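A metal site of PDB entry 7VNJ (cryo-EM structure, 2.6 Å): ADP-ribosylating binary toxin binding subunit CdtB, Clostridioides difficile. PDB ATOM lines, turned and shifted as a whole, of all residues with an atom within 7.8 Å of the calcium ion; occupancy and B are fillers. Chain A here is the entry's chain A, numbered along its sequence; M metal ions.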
ATOM      1  N   PHE A 418      21.333  20.593  21.396  1.00  0.00           N
ATOM      2  CA  PHE A 418      22.651  20.369  20.839  1.00  0.00           C
ATOM      3  C   PHE A 418      22.578  19.272  19.795  1.00  0.00           C
ATOM      4  O   PHE A 418      21.762  18.351  19.889  1.00  0.00           O
ATOM      5  CB  PHE A 418      23.643  19.991  21.953  1.00  0.00           C
ATOM      6  CG  PHE A 418      24.999  19.585  21.451  1.00  0.00           C
ATOM      7  CD1 PHE A 418      25.919  20.526  21.063  1.00  0.00           C
ATOM      8  CD2 PHE A 418      25.340  18.244  21.387  1.00  0.00           C
ATOM      9  CE1 PHE A 418      27.173  20.147  20.604  1.00  0.00           C
ATOM     10  CE2 PHE A 418      26.584  17.856  20.927  1.00  0.00           C
ATOM     11  CZ  PHE A 418      27.498  18.805  20.539  1.00  0.00           C
ATOM     12  N   THR A 419      23.448  19.369  18.797  1.00  0.00           N
ATOM     13  CA  THR A 419      23.585  18.318  17.797  1.00  0.00           C
ATOM     14  C   THR A 419      25.001  18.337  17.242  1.00  0.00           C
ATOM     15  O   THR A 419      25.569  19.412  17.015  1.00  0.00           O
ATOM     16  CB  THR A 419      22.563  18.459  16.669  1.00  0.00           C
ATOM     17  OG1 THR A 419      22.718  17.379  15.737  1.00  0.00           O
ATOM     18  CG2 THR A 419      22.715  19.781  15.938  1.00  0.00           C
ATOM     19  N   ASN A 420      25.564  17.158  17.033  1.00  0.00           N
ATOM     20  CA  ASN A 420      26.877  17.000  16.418  1.00  0.00           C
ATOM     21  C   ASN A 420      26.784  16.538  14.976  1.00  0.00           C
ATOM     22  O   ASN A 420      27.820  16.314  14.336  1.00  0.00           O
ATOM     23  CB  ASN A 420      27.724  16.018  17.219  1.00  0.00           C
ATOM     24  CG  ASN A 420      26.975  14.751  17.567  1.00  0.00           C
ATOM     25  OD1 ASN A 420      25.833  14.552  17.138  1.00  0.00           O
ATOM     26  ND2 ASN A 420      27.616  13.872  18.338  1.00  0.00           N
ATOM     27  N   PHE A 421      25.566  16.386  14.443  1.00  0.00           N
ATOM     28  CA  PHE A 421      25.306  15.891  13.095  1.00  0.00           C
ATOM     29  C   PHE A 421      25.882  14.501  12.853  1.00  0.00           C
ATOM     30  O   PHE A 421      26.000  14.067  11.701  1.00  0.00           O
ATOM     31  CB  PHE A 421      25.847  16.860  12.027  1.00  0.00           C
ATOM     32  CG  PHE A 421      25.447  18.284  12.247  1.00  0.00           C
ATOM     33  CD1 PHE A 421      24.112  18.650  12.305  1.00  0.00           C
ATOM     34  CD2 PHE A 421      26.419  19.271  12.381  1.00  0.00           C
ATOM     35  CE1 PHE A 421      23.752  19.965  12.501  1.00  0.00           C
ATOM     36  CE2 PHE A 421      26.052  20.594  12.579  1.00  0.00           C
ATOM     37  CZ  PHE A 421      24.720  20.935  12.635  1.00  0.00           C
ATOM     38  N   ASP A 422      26.252  13.776  13.916  1.00  0.00           N
ATOM     39  CA  ASP A 422      26.776  12.426  13.783  1.00  0.00           C
ATOM     40  C   ASP A 422      25.847  11.394  14.398  1.00  0.00           C
ATOM     41  O   ASP A 422      25.381  10.489  13.698  1.00  0.00           O
ATOM     42  CB  ASP A 422      28.164  12.345  14.441  1.00  0.00           C
ATOM     43  CG  ASP A 422      29.159  13.301  13.820  1.00  0.00           C
ATOM     44  OD1 ASP A 422      29.232  13.363  12.585  1.00  0.00           O
ATOM     45  OD2 ASP A 422      29.875  13.982  14.583  1.00  0.00           O
ATOM     46  N   ASP A 423      25.564  11.505  15.688  1.00  0.00           N
ATOM     47  CA  ASP A 423      24.634  10.588  16.348  1.00  0.00           C
ATOM     48  C   ASP A 423      23.674  11.275  17.316  1.00  0.00           C
ATOM     49  O   ASP A 423      22.618  10.701  17.593  1.00  0.00           O
ATOM     50  CB  ASP A 423      25.395   9.494  17.109  1.00  0.00           C
ATOM     51  CG  ASP A 423      26.405  10.068  18.095  1.00  0.00           C
ATOM     52  OD1 ASP A 423      26.628  11.293  18.081  1.00  0.00           O
ATOM     53  OD2 ASP A 423      26.962   9.286  18.887  1.00  0.00           O
ATOM     54  N   ASP A 440      34.525  15.893   7.555  1.00  0.00           N
ATOM     55  CA  ASP A 440      35.021  17.139   8.109  1.00  0.00           C
ATOM     56  C   ASP A 440      34.351  17.401   9.455  1.00  0.00           C
ATOM     57  O   ASP A 440      33.443  16.692   9.886  1.00  0.00           O
ATOM     58  CB  ASP A 440      34.776  18.295   7.143  1.00  0.00           C
ATOM     59  CG  ASP A 440      35.529  18.128   5.835  1.00  0.00           C
ATOM     60  OD1 ASP A 440      36.694  17.689   5.867  1.00  0.00           O
ATOM     61  OD2 ASP A 440      34.948  18.433   4.780  1.00  0.00           O
ATOM     62  N   GLY A 441      34.810  18.448  10.125  1.00  0.00           N
ATOM     63  CA  GLY A 441      34.253  18.825  11.413  1.00  0.00           C
ATOM     64  C   GLY A 441      35.041  18.255  12.569  1.00  0.00           C
ATOM     65  O   GLY A 441      36.025  17.515  12.407  1.00  0.00           O
ATOM     66  N   LEU A 442      34.578  18.586  13.776  1.00  0.00           N
ATOM     67  CA  LEU A 442      35.254  18.141  14.984  1.00  0.00           C
ATOM     68  C   LEU A 442      35.189  16.620  15.123  1.00  0.00           C
ATOM     69  O   LEU A 442      36.153  15.991  15.553  1.00  0.00           O
ATOM     70  CB  LEU A 442      34.637  18.814  16.212  1.00  0.00           C
ATOM     71  CG  LEU A 442      35.128  20.215  16.595  1.00  0.00           C
ATOM     72  CD1 LEU A 442      36.606  20.193  16.947  1.00  0.00           C
ATOM     73  CD2 LEU A 442      34.852  21.247  15.504  1.00  0.00           C
ATOM     74  N   GLN A 443      34.049  16.020  14.758  1.00  0.00           N
ATOM     75  CA  GLN A 443      33.901  14.575  14.888  1.00  0.00           C
ATOM     76  C   GLN A 443      33.215  13.953  13.676  1.00  0.00           C
ATOM     77  O   GLN A 443      32.498  12.954  13.808  1.00  0.00           O
ATOM     78  CB  GLN A 443      33.129  14.224  16.163  1.00  0.00           C
ATOM     79  CG  GLN A 443      33.952  14.298  17.434  1.00  0.00           C
ATOM     80  CD  GLN A 443      33.906  15.664  18.089  1.00  0.00           C
ATOM     81  OE1 GLN A 443      32.947  16.424  17.905  1.00  0.00           O
ATOM     82  NE2 GLN A 443      34.945  16.001  18.848  1.00  0.00           N
ATOM     83  N   GLY A 444      33.425  14.526  12.489  1.00  0.00           N
ATOM     84  CA  GLY A 444      32.971  13.894  11.267  1.00  0.00           C
ATOM     85  C   GLY A 444      31.654  14.374  10.696  1.00  0.00           C
ATOM     86  O   GLY A 444      30.818  13.564  10.296  1.00  0.00           O
ATOM     87  N   SER A 445      31.463  15.695  10.641  1.00  0.00           N
ATOM     88  CA  SER A 445      30.247  16.262  10.073  1.00  0.00           C
ATOM     89  C   SER A 445      30.472  17.734   9.783  1.00  0.00           C
ATOM     90  O   SER A 445      31.213  18.412  10.504  1.00  0.00           O
ATOM     91  CB  SER A 445      29.050  16.086  11.008  1.00  0.00           C
ATOM     92  OG  SER A 445      29.270  16.726  12.255  1.00  0.00           O
ATOM     93  N   ALA A 446      29.840  18.220   8.721  1.00  0.00           N
ATOM     94  CA  ALA A 446      30.007  19.600   8.280  1.00  0.00           C
ATOM     95  C   ALA A 446      28.702  20.372   8.198  1.00  0.00           C
ATOM     96  O   ALA A 446      28.663  21.537   8.621  1.00  0.00           O
ATOM     97  CB  ALA A 446      30.702  19.625   6.925  1.00  0.00           C
ATOM     98  N   TYR A 503      39.199  25.626  13.605  1.00  0.00           N
ATOM     99  CA  TYR A 503      37.876  25.845  14.168  1.00  0.00           C
ATOM    100  C   TYR A 503      37.932  26.840  15.317  1.00  0.00           C
ATOM    101  O   TYR A 503      38.941  26.958  16.013  1.00  0.00           O
ATOM    102  CB  TYR A 503      37.254  24.532  14.664  1.00  0.00           C
ATOM    103  CG  TYR A 503      36.469  23.800  13.604  1.00  0.00           C
ATOM    104  CD1 TYR A 503      35.197  24.225  13.242  1.00  0.00           C
ATOM    105  CD2 TYR A 503      36.985  22.678  12.973  1.00  0.00           C
ATOM    106  CE1 TYR A 503      34.467  23.561  12.282  1.00  0.00           C
ATOM    107  CE2 TYR A 503      36.261  22.006  12.012  1.00  0.00           C
ATOM    108  CZ  TYR A 503      35.004  22.456  11.667  1.00  0.00           C
ATOM    109  OH  TYR A 503      34.261  21.806  10.708  1.00  0.00           O
ATOM    110  N   LEU A 532      30.472  23.701   9.573  1.00  0.00           N
ATOM    111  CA  LEU A 532      29.856  23.894  10.878  1.00  0.00           C
ATOM    112  C   LEU A 532      29.816  22.561  11.617  1.00  0.00           C
ATOM    113  O   LEU A 532      29.822  21.487  11.010  1.00  0.00           O
ATOM    114  CB  LEU A 532      28.441  24.480  10.770  1.00  0.00           C
ATOM    115  CG  LEU A 532      28.327  25.946  10.360  1.00  0.00           C
ATOM    116  CD1 LEU A 532      26.877  26.357  10.249  1.00  0.00           C
ATOM    117  CD2 LEU A 532      29.065  26.840  11.341  1.00  0.00           C
ATOM    118  N   ASP A 533      29.761  22.640  12.951  1.00  0.00           N
ATOM    119  CA  ASP A 533      29.670  21.454  13.794  1.00  0.00           C
ATOM    120  C   ASP A 533      29.359  21.888  15.212  1.00  0.00           C
ATOM    121  O   ASP A 533      29.744  22.982  15.644  1.00  0.00           O
ATOM    122  CB  ASP A 533      30.960  20.626  13.758  1.00  0.00           C
ATOM    123  CG  ASP A 533      30.697  19.136  13.832  1.00  0.00           C
ATOM    124  OD1 ASP A 533      29.518  18.745  13.953  1.00  0.00           O
ATOM    125  OD2 ASP A 533      31.665  18.350  13.758  1.00  0.00           O
ATOM    126  N   ASN A 534      28.662  21.008  15.944  1.00  0.00           N
ATOM    127  CA  ASN A 534      28.392  21.186  17.375  1.00  0.00           C
ATOM    128  C   ASN A 534      27.648  22.495  17.642  1.00  0.00           C
ATOM    129  O   ASN A 534      28.150  23.393  18.322  1.00  0.00           O
ATOM    130  CB  ASN A 534      29.684  21.101  18.194  1.00  0.00           C
ATOM    131  CG  ASN A 534      30.364  19.753  18.071  1.00  0.00           C
ATOM    132  OD1 ASN A 534      29.699  18.731  17.875  1.00  0.00           O
ATOM    133  ND2 ASN A 534      31.678  19.741  18.186  1.00  0.00           N
ATOM    134  N   LEU A 535      26.441  22.592  17.104  1.00  0.00           N
ATOM    135  CA  LEU A 535      25.580  23.737  17.325  1.00  0.00           C
ATOM    136  C   LEU A 535      24.771  23.528  18.591  1.00  0.00           C
ATOM    137  O   LEU A 535      24.104  22.492  18.735  1.00  0.00           O
ATOM    138  CB  LEU A 535      24.656  23.980  16.130  1.00  0.00           C
ATOM    139  CG  LEU A 535      25.339  24.193  14.777  1.00  0.00           C
ATOM    140  CD1 LEU A 535      24.306  24.505  13.714  1.00  0.00           C
ATOM    141  CD2 LEU A 535      26.364  25.308  14.875  1.00  0.00           C
HETATM  142 CA    CA M   1      30.304  16.452  14.437  1.00  0.00          CA
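N of Gln 443 touches the calcium ion, 3.8 Å away.
The backbone NH (N) of Gln 443 sits close to the side-chain carboxylate (OD2) of Asp 533 (3.5 Å). OD2 of Asp 533 sits close to N of Leu 442 (2.9 Å). The side-chain amide nitrogen of Asn 420 is in hydrogen-bond range of the side-chain carboxylate of Asp 423.
The calcium ion is bound by OG of Ser 445 (2.4 Å), OD2 of Asp 533 (2.4 Å), OD1 of Asp 533 (2.5 Å), O of Asn 420 (2.5 Å) and OD2 of Asp 422 (2.5 Å). The calcium ion has five donor atoms within binding distance.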
